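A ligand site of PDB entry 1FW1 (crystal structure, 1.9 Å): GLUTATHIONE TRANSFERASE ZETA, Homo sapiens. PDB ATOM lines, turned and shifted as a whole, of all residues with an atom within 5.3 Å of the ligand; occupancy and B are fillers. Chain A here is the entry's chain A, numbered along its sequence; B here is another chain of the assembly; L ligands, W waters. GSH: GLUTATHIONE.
An oxygen (O11) of the ligand lies within hydrogen-bond range of the backbone NH (N) of Ser 72 (2.8 Å). The side-chain hydroxyl (OG) of Ser 72 sits at hydrogen-bond distance from an oxygen (O12) of the ligand (2.5 Å). The backbone NH of Cys 16 lies close to a sulfur (SG2) of the ligand (3.5 Å). SG2 of the ligand lies close to SG of Cys 16 (2.8 Å). A nitrogen (N1) of the ligand sits at hydrogen-bond distance from the side-chain amide oxygen (OE1) of Gln 71 (2.8 Å). N of Ser 117 is in hydrogen-bond range of O32 of the ligand (2.8 Å). N of Val 59 sits at hydrogen-bond distance from O2 of the ligand (2.9 Å). A nitrogen (N2) of the ligand is in hydrogen-bond range of the backbone carbonyl oxygen (O) of Val 59 (2.9 Å). The side-chain amide nitrogen (NE2) of Gln 45 sits at hydrogen-bond distance from an oxygen (O31) of the ligand (2.9 Å). NH1 of Arg 19 is in salt-bridge range of O12 of the ligand. The side-chain amide nitrogen of Asn 115 sits at hydrogen-bond distance from an oxygen (O32) of the ligand (3.2 Å). SG2 of the ligand lies close to NE2 of Gln 111 (3.5 Å).
The side-chain hydroxyl (OG) of Ser 72 is in hydrogen-bond range of the guanidinium group (NH1) of Arg 19, 2.8 Å away. SG of Cys 16 lies within hydrogen-bond range of NH1 of Arg 19 (3.8 Å). The side-chain amide oxygen (OE1) of Gln 111 sits close to the side-chain sulfur (SG) of Cys 16. The side-chain hydroxyl (OG) of Ser 117 sits at hydrogen-bond distance from the side-chain amide nitrogen (ND2) of Asn 115 (3.2 Å). The side-chain amide nitrogen of Gln 45 is in hydrogen-bond range of the backbone carbonyl oxygen of Leu 38, at 3.2 Å. NE2 of Gln 111 lies within hydrogen-bond range of OD1 of Asn 115, 3.3 Å away. OG of Ser 14 sits at hydrogen-bond distance from OG of Ser 17 (2.7 Å).
Residues that only touch the ligand: Gln 58, Ser 14, Leu 116, Leu 38, Pro 60, Ser 15, Lys 57 and Phe 46. Hydrophobic or aromatic side chains that line the ligand: Leu 38, Phe 46, Val 59, Pro 60 and Leu 116. Within 4 Å of the ligand: Ser 14, Ser 15, Cys 16, Arg 19, Leu 38, Gln 45, Phe 46, Lys 57, Gln 58, Val 59, Pro 60, Gln 71, Ser 72, Gln 111, Asn 115, Leu 116 and Ser 117. The nearest printed residue that does not touch the ligand is Ala 107 (4.4 Å).
Water W5 bridges OE1 of the ligand (2.5 Å) and OE1 of Gln 111 (2.9 Å). Water W1 bridges O of Lys 57 (2.8 Å) and O31 of the ligand (2.8 Å). Water W4 lies within hydrogen-bond range of O of Pro 60 (2.7 Å), O11 of the ligand (2.9 Å) and N of Gln 71 (3.0 Å). Water W9 lies within hydrogen-bond range of O of Ala 107 and N1 of the ligand. Water W3 lies within hydrogen-bond range of OD2 of Asp 104 of chain B (2.9 Å), N of Leu 73 (3.0 Å), O12 of the ligand (3.0 Å), OE1 of Gln 71 (3.1 Å) and N of Ser 72 (3.3 Å). Water W2 lies within hydrogen-bond range of the side-chain amide nitrogen of Gln 58 (3.0 Å), the side-chain hydroxyl of Ser 117 (3.0 Å), the side-chain amide nitrogen of Asn 115 (3.1 Å) and an oxygen (O32) of the ligand (3.4 Å).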
ATOM      1  N   SER A  14      -0.064 -14.733  19.121  1.00  0.00           N
ATOM      2  CA  SER A  14       1.112 -15.569  19.257  1.00  0.00           C
ATOM      3  C   SER A  14       0.944 -16.823  18.432  1.00  0.00           C
ATOM      4  O   SER A  14      -0.095 -17.497  18.496  1.00  0.00           O
ATOM      5  CB  SER A  14       1.399 -15.886  20.722  1.00  0.00           C
ATOM      6  OG  SER A  14       0.280 -16.474  21.331  1.00  0.00           O
ATOM      7  N   SER A  15       1.951 -17.121  17.616  1.00  0.00           N
ATOM      8  CA  SER A  15       1.817 -18.290  16.766  1.00  0.00           C
ATOM      9  C   SER A  15       1.752 -19.539  17.644  1.00  0.00           C
ATOM     10  O   SER A  15       0.968 -20.416  17.359  1.00  0.00           O
ATOM     11  CB  SER A  15       3.012 -18.372  15.761  1.00  0.00           C
ATOM     12  OG  SER A  15       4.198 -18.544  16.490  1.00  0.00           O
ATOM     13  N   CYS A  16       2.552 -19.613  18.709  1.00  0.00           N
ATOM     14  CA  CYS A  16       2.578 -20.794  19.570  1.00  0.00           C
ATOM     15  C   CYS A  16       1.222 -21.126  20.194  1.00  0.00           C
ATOM     16  O   CYS A  16       0.880 -22.307  20.369  1.00  0.00           O
ATOM     17  CB  CYS A  16       3.619 -20.634  20.691  1.00  0.00           C
ATOM     18  SG  CYS A  16       5.284 -20.143  20.105  1.00  0.00           S
ATOM     19  N   SER A  17       0.459 -20.089  20.526  1.00  0.00           N
ATOM     20  CA  SER A  17      -0.848 -20.305  21.116  1.00  0.00           C
ATOM     21  C   SER A  17      -1.797 -20.770  20.042  1.00  0.00           C
ATOM     22  O   SER A  17      -2.594 -21.654  20.262  1.00  0.00           O
ATOM     23  CB  SER A  17      -1.411 -18.988  21.724  1.00  0.00           C
ATOM     24  OG  SER A  17      -0.644 -18.578  22.838  1.00  0.00           O
ATOM     25  N   ARG A  19      -1.296 -22.655  17.616  1.00  0.00           N
ATOM     26  CA  ARG A  19      -1.133 -24.118  17.393  1.00  0.00           C
ATOM     27  C   ARG A  19      -2.038 -24.920  18.348  1.00  0.00           C
ATOM     28  O   ARG A  19      -2.690 -25.872  17.929  1.00  0.00           O
ATOM     29  CB  ARG A  19       0.300 -24.579  17.680  1.00  0.00           C
ATOM     30  CG  ARG A  19       1.370 -23.777  16.940  1.00  0.00           C
ATOM     31  CD  ARG A  19       2.788 -24.260  17.409  1.00  0.00           C
ATOM     32  NE  ARG A  19       3.864 -23.460  16.860  1.00  0.00           N
ATOM     33  CZ  ARG A  19       4.993 -23.193  17.515  1.00  0.00           C
ATOM     34  NH1 ARG A  19       5.182 -23.666  18.741  1.00  0.00           N
ATOM     35  NH2 ARG A  19       5.925 -22.449  16.951  1.00  0.00           N
ATOM     36  N   LEU A  38       1.236  -9.992  25.620  1.00  0.00           N
ATOM     37  CA  LEU A  38       2.689 -10.051  25.528  1.00  0.00           C
ATOM     38  C   LEU A  38       3.392  -8.742  25.220  1.00  0.00           C
ATOM     39  O   LEU A  38       4.634  -8.673  25.316  1.00  0.00           O
ATOM     40  CB  LEU A  38       3.118 -11.117  24.503  1.00  0.00           C
ATOM     41  CG  LEU A  38       2.561 -12.532  24.702  1.00  0.00           C
ATOM     42  CD1 LEU A  38       3.040 -13.450  23.555  1.00  0.00           C
ATOM     43  CD2 LEU A  38       2.985 -13.099  26.038  1.00  0.00           C
ATOM     44  N   GLN A  45       3.551 -11.419  30.601  1.00  0.00           N
ATOM     45  CA  GLN A  45       4.332 -12.649  30.732  1.00  0.00           C
ATOM     46  C   GLN A  45       5.424 -12.486  31.772  1.00  0.00           C
ATOM     47  O   GLN A  45       6.069 -13.456  32.141  1.00  0.00           O
ATOM     48  CB  GLN A  45       4.958 -13.138  29.392  1.00  0.00           C
ATOM     49  CG  GLN A  45       6.104 -12.283  28.811  1.00  0.00           C
ATOM     50  CD  GLN A  45       5.599 -11.178  27.914  1.00  0.00           C
ATOM     51  OE1 GLN A  45       4.610 -10.521  28.232  1.00  0.00           O
ATOM     52  NE2 GLN A  45       6.272 -10.956  26.790  1.00  0.00           N
ATOM     53  N   PHE A  46       5.616 -11.273  32.256  1.00  0.00           N
ATOM     54  CA  PHE A  46       6.643 -11.002  33.260  1.00  0.00           C
ATOM     55  C   PHE A  46       6.060 -10.633  34.639  1.00  0.00           C
ATOM     56  O   PHE A  46       6.793 -10.520  35.622  1.00  0.00           O
ATOM     57  CB  PHE A  46       7.564  -9.890  32.757  1.00  0.00           C
ATOM     58  CG  PHE A  46       8.342 -10.276  31.539  1.00  0.00           C
ATOM     59  CD1 PHE A  46       8.164  -9.601  30.341  1.00  0.00           C
ATOM     60  CD2 PHE A  46       9.224 -11.336  31.571  1.00  0.00           C
ATOM     61  CE1 PHE A  46       8.849  -9.973  29.193  1.00  0.00           C
ATOM     62  CE2 PHE A  46       9.915 -11.730  30.412  1.00  0.00           C
ATOM     63  CZ  PHE A  46       9.723 -11.038  29.220  1.00  0.00           C
ATOM     64  N   LYS A  57       7.942 -17.896  31.184  1.00  0.00           N
ATOM     65  CA  LYS A  57       7.257 -16.641  30.808  1.00  0.00           C
ATOM     66  C   LYS A  57       6.860 -16.589  29.338  1.00  0.00           C
ATOM     67  O   LYS A  57       7.153 -15.632  28.611  1.00  0.00           O
ATOM     68  CB  LYS A  57       8.155 -15.446  31.147  1.00  0.00           C
ATOM     69  CG  LYS A  57       8.659 -15.478  32.620  1.00  0.00           C
ATOM     70  CD  LYS A  57       9.706 -14.412  32.886  1.00  0.00           C
ATOM     71  CE  LYS A  57      10.669 -14.808  34.004  1.00  0.00           C
ATOM     72  NZ  LYS A  57      11.773 -13.792  34.188  1.00  0.00           N
ATOM     73  N   GLN A  58       6.130 -17.601  28.929  1.00  0.00           N
ATOM     74  CA  GLN A  58       5.696 -17.698  27.563  1.00  0.00           C
ATOM     75  C   GLN A  58       4.312 -18.317  27.556  1.00  0.00           C
ATOM     76  O   GLN A  58       3.913 -18.947  28.521  1.00  0.00           O
ATOM     77  CB  GLN A  58       6.670 -18.647  26.799  1.00  0.00           C
ATOM     78  CG  GLN A  58       8.115 -18.135  26.685  1.00  0.00           C
ATOM     79  CD  GLN A  58       9.125 -19.222  26.147  1.00  0.00           C
ATOM     80  OE1 GLN A  58       8.891 -20.432  26.264  1.00  0.00           O
ATOM     81  NE2 GLN A  58      10.264 -18.767  25.642  1.00  0.00           N
ATOM     82  N   VAL A  59       3.582 -18.138  26.457  1.00  0.00           N
ATOM     83  CA  VAL A  59       2.305 -18.764  26.274  1.00  0.00           C
ATOM     84  C   VAL A  59       2.567 -19.668  25.061  1.00  0.00           C
ATOM     85  O   VAL A  59       3.322 -19.305  24.172  1.00  0.00           O
ATOM     86  CB  VAL A  59       1.147 -17.766  25.970  1.00  0.00           C
ATOM     87  CG1 VAL A  59       0.727 -17.039  27.275  1.00  0.00           C
ATOM     88  CG2 VAL A  59       1.560 -16.755  24.936  1.00  0.00           C
ATOM     89  N   PRO A  60       1.813 -20.753  24.930  1.00  0.00           N
ATOM     90  CA  PRO A  60       0.715 -21.220  25.804  1.00  0.00           C
ATOM     91  C   PRO A  60       1.092 -22.116  26.953  1.00  0.00           C
ATOM     92  O   PRO A  60       2.165 -22.728  26.991  1.00  0.00           O
ATOM     93  CB  PRO A  60      -0.173 -21.964  24.840  1.00  0.00           C
ATOM     94  CG  PRO A  60       0.918 -22.728  23.981  1.00  0.00           C
ATOM     95  CD  PRO A  60       1.993 -21.662  23.764  1.00  0.00           C
ATOM     96  N   GLN A  71       4.679 -25.763  26.798  1.00  0.00           N
ATOM     97  CA  GLN A  71       5.274 -26.269  25.520  1.00  0.00           C
ATOM     98  C   GLN A  71       4.186 -26.776  24.592  1.00  0.00           C
ATOM     99  O   GLN A  71       3.538 -27.836  24.840  1.00  0.00           O
ATOM    100  CB  GLN A  71       6.336 -27.322  25.776  1.00  0.00           C
ATOM    101  CG  GLN A  71       7.571 -26.743  26.480  1.00  0.00           C
ATOM    102  CD  GLN A  71       8.311 -25.698  25.646  1.00  0.00           C
ATOM    103  OE1 GLN A  71       8.257 -25.685  24.414  1.00  0.00           O
ATOM    104  NE2 GLN A  71       9.040 -24.812  26.347  1.00  0.00           N
ATOM    105  N   SER A  72       3.937 -25.968  23.565  1.00  0.00           N
ATOM    106  CA  SER A  72       2.852 -26.222  22.634  1.00  0.00           C
ATOM    107  C   SER A  72       2.824 -27.652  22.110  1.00  0.00           C
ATOM    108  O   SER A  72       1.773 -28.237  22.094  1.00  0.00           O
ATOM    109  CB  SER A  72       2.880 -25.211  21.476  1.00  0.00           C
ATOM    110  OG  SER A  72       4.071 -25.315  20.716  1.00  0.00           O
ATOM    111  N   LEU A  73       3.949 -28.226  21.696  1.00  0.00           N
ATOM    112  CA  LEU A  73       3.901 -29.577  21.175  1.00  0.00           C
ATOM    113  C   LEU A  73       3.686 -30.605  22.289  1.00  0.00           C
ATOM    114  O   LEU A  73       2.991 -31.602  22.074  1.00  0.00           O
ATOM    115  CB  LEU A  73       5.192 -29.902  20.357  1.00  0.00           C
ATOM    116  CG  LEU A  73       5.528 -28.886  19.252  1.00  0.00           C
ATOM    117  CD1 LEU A  73       6.757 -29.409  18.398  1.00  0.00           C
ATOM    118  CD2 LEU A  73       4.302 -28.643  18.342  1.00  0.00           C
ATOM    119  N   ALA A 107       8.683 -25.229  15.089  1.00  0.00           N
ATOM    120  CA  ALA A 107       8.621 -24.817  16.508  1.00  0.00           C
ATOM    121  C   ALA A 107       9.913 -24.660  17.273  1.00  0.00           C
ATOM    122  O   ALA A 107       9.967 -23.898  18.275  1.00  0.00           O
ATOM    123  CB  ALA A 107       7.702 -25.745  17.291  1.00  0.00           C
ATOM    124  N   GLN A 111      10.582 -20.502  14.731  1.00  0.00           N
ATOM    125  CA  GLN A 111       9.917 -19.611  15.662  1.00  0.00           C
ATOM    126  C   GLN A 111      10.799 -19.021  16.769  1.00  0.00           C
ATOM    127  O   GLN A 111      10.752 -17.826  16.986  1.00  0.00           O
ATOM    128  CB  GLN A 111       8.705 -20.283  16.283  1.00  0.00           C
ATOM    129  CG  GLN A 111       7.771 -19.296  17.013  1.00  0.00           C
ATOM    130  CD  GLN A 111       8.255 -18.926  18.429  1.00  0.00           C
ATOM    131  OE1 GLN A 111       8.830 -19.758  19.166  1.00  0.00           O
ATOM    132  NE2 GLN A 111       8.016 -17.690  18.821  1.00  0.00           N
ATOM    133  N   ASN A 115      11.164 -15.027  17.970  1.00  0.00           N
ATOM    134  CA  ASN A 115      10.383 -14.846  19.188  1.00  0.00           C
ATOM    135  C   ASN A 115      10.602 -13.407  19.697  1.00  0.00           C
ATOM    136  O   ASN A 115      11.710 -12.873  19.630  1.00  0.00           O
ATOM    137  CB  ASN A 115      10.857 -15.877  20.228  1.00  0.00           C
ATOM    138  CG  ASN A 115      10.030 -15.859  21.517  1.00  0.00           C
ATOM    139  OD1 ASN A 115       8.816 -15.862  21.502  1.00  0.00           O
ATOM    140  ND2 ASN A 115      10.721 -15.896  22.652  1.00  0.00           N
ATOM    141  N   LEU A 116       9.534 -12.791  20.209  1.00  0.00           N
ATOM    142  CA  LEU A 116       9.595 -11.424  20.716  1.00  0.00           C
ATOM    143  C   LEU A 116      10.799 -11.096  21.606  1.00  0.00           C
ATOM    144  O   LEU A 116      11.530 -10.127  21.350  1.00  0.00           O
ATOM    145  CB  LEU A 116       8.280 -11.098  21.490  1.00  0.00           C
ATOM    146  CG  LEU A 116       8.287  -9.656  22.014  1.00  0.00           C
ATOM    147  CD1 LEU A 116       8.212  -8.712  20.810  1.00  0.00           C
ATOM    148  CD2 LEU A 116       7.088  -9.414  23.027  1.00  0.00           C
ATOM    149  N   SER A 117      11.041 -11.892  22.632  1.00  0.00           N
ATOM    150  CA  SER A 117      12.145 -11.619  23.538  1.00  0.00           C
ATOM    151  C   SER A 117      13.506 -11.699  22.863  1.00  0.00           C
ATOM    152  O   SER A 117      14.462 -11.095  23.325  1.00  0.00           O
ATOM    153  CB  SER A 117      12.088 -12.540  24.762  1.00  0.00           C
ATOM    154  OG  SER A 117      12.480 -13.867  24.439  1.00  0.00           O
ATOM    155  N   VAL A 118      13.615 -12.452  21.768  1.00  0.00           N
ATOM    156  CA  VAL A 118      14.903 -12.501  21.055  1.00  0.00           C
ATOM    157  C   VAL A 118      14.955 -11.228  20.177  1.00  0.00           C
ATOM    158  O   VAL A 118      15.980 -10.537  20.119  1.00  0.00           O
ATOM    159  CB  VAL A 118      14.994 -13.763  20.189  1.00  0.00           C
ATOM    160  CG1 VAL A 118      16.196 -13.685  19.255  1.00  0.00           C
ATOM    161  CG2 VAL A 118      15.095 -14.974  21.105  1.00  0.00           C
ATOM    162  N   LYS A 120      13.659  -8.408  20.786  1.00  0.00           N
ATOM    163  CA  LYS A 120      13.950  -7.255  21.654  1.00  0.00           C
ATOM    164  C   LYS A 120      15.456  -7.125  21.860  1.00  0.00           C
ATOM    165  O   LYS A 120      15.975  -6.004  21.873  1.00  0.00           O
ATOM    166  CB  LYS A 120      13.247  -7.377  23.018  1.00  0.00           C
ATOM    167  CG  LYS A 120      11.757  -6.926  23.026  1.00  0.00           C
ATOM    168  CD  LYS A 120      11.020  -7.328  24.362  1.00  0.00           C
ATOM    169  CE  LYS A 120       9.545  -6.852  24.384  1.00  0.00           C
ATOM    170  NZ  LYS A 120       8.729  -7.390  25.537  1.00  0.00           N
ATOM    171  N   ASP B 104      11.225 -30.209  25.167  1.00  0.00           N
ATOM    172  CA  ASP B 104      11.012 -29.061  24.292  1.00  0.00           C
ATOM    173  C   ASP B 104      11.582 -27.788  24.878  1.00  0.00           C
ATOM    174  O   ASP B 104      12.049 -26.928  24.132  1.00  0.00           O
ATOM    175  CB  ASP B 104       9.520 -28.844  24.007  1.00  0.00           C
ATOM    176  CG  ASP B 104       8.955 -29.861  23.052  1.00  0.00           C
ATOM    177  OD1 ASP B 104       9.739 -30.758  22.589  1.00  0.00           O
ATOM    178  OD2 ASP B 104       7.736 -29.782  22.755  1.00  0.00           O
ATOM    179  N   GLY B 108      14.069 -26.657  22.222  1.00  0.00           N
ATOM    180  CA  GLY B 108      13.438 -25.621  21.454  1.00  0.00           C
ATOM    181  C   GLY B 108      13.490 -24.249  22.130  1.00  0.00           C
ATOM    182  O   GLY B 108      13.363 -23.228  21.459  1.00  0.00           O
ATOM    183  N   GLY B 109      13.657 -24.230  23.444  1.00  0.00           N
ATOM    184  CA  GLY B 109      13.690 -22.957  24.156  1.00  0.00           C
ATOM    185  C   GLY B 109      15.018 -22.435  24.672  1.00  0.00           C
ATOM    186  O   GLY B 109      15.108 -21.256  25.118  1.00  0.00           O
HETATM  187  N1  GSH L   1       8.635 -23.743  22.446  1.00  0.00           N
HETATM  188  CA1 GSH L   1       7.551 -22.971  23.107  1.00  0.00           C
HETATM  189  C1  GSH L   1       6.165 -23.565  22.681  1.00  0.00           C
HETATM  190  O11 GSH L   1       5.215 -23.453  23.533  1.00  0.00           O
HETATM  191  O12 GSH L   1       6.174 -24.235  21.647  1.00  0.00           O
HETATM  192  CB1 GSH L   1       7.675 -21.455  22.690  1.00  0.00           C
HETATM  193  CG1 GSH L   1       6.579 -20.543  23.350  1.00  0.00           C
HETATM  194  CD1 GSH L   1       6.881 -19.011  23.232  1.00  0.00           C
HETATM  195  OE1 GSH L   1       7.964 -18.726  22.678  1.00  0.00           O
HETATM  196  N2  GSH L   1       5.815 -18.231  23.259  1.00  0.00           N
HETATM  197  CA2 GSH L   1       5.786 -16.927  22.634  1.00  0.00           C
HETATM  198  C2  GSH L   1       5.726 -15.918  23.774  1.00  0.00           C
HETATM  199  O2  GSH L   1       5.014 -16.172  24.845  1.00  0.00           O
HETATM  200  CB2 GSH L   1       4.489 -16.633  21.808  1.00  0.00           C
HETATM  201  SG2 GSH L   1       4.775 -17.408  20.226  1.00  0.00           S
HETATM  202  N3  GSH L   1       6.868 -15.198  23.938  1.00  0.00           N
HETATM  203  CA3 GSH L   1       6.980 -14.175  25.007  1.00  0.00           C
HETATM  204  C3  GSH L   1       8.115 -13.182  24.743  1.00  0.00           C
HETATM  205  O31 GSH L   1       8.490 -12.507  25.778  1.00  0.00           O
HETATM  206  O32 GSH L   1       9.047 -13.491  23.869  1.00  0.00           O
HETATM  207  O   HOH W   1       9.475 -14.289  27.741  1.00  0.00           O
HETATM  208  O   HOH W   2      10.594 -15.793  25.757  1.00  0.00           O
HETATM  209  O   HOH W   3       6.692 -27.174  22.169  1.00  0.00           O
HETATM  210  O   HOH W   4       4.801 -22.779  26.296  1.00  0.00           O
HETATM  211  O   HOH W   5      10.194 -19.345  21.663  1.00  0.00           O
HETATM  212  O   HOH W   6      10.293 -22.342  25.008  1.00  0.00           O
HETATM  213  O   HOH W   7      10.003 -10.109  25.393  1.00  0.00           O
HETATM  214  O   HOH W   8      11.083 -22.072  22.284  1.00  0.00           O
HETATM  215  O   HOH W   9      10.282 -25.031  20.463  1.00  0.00           O
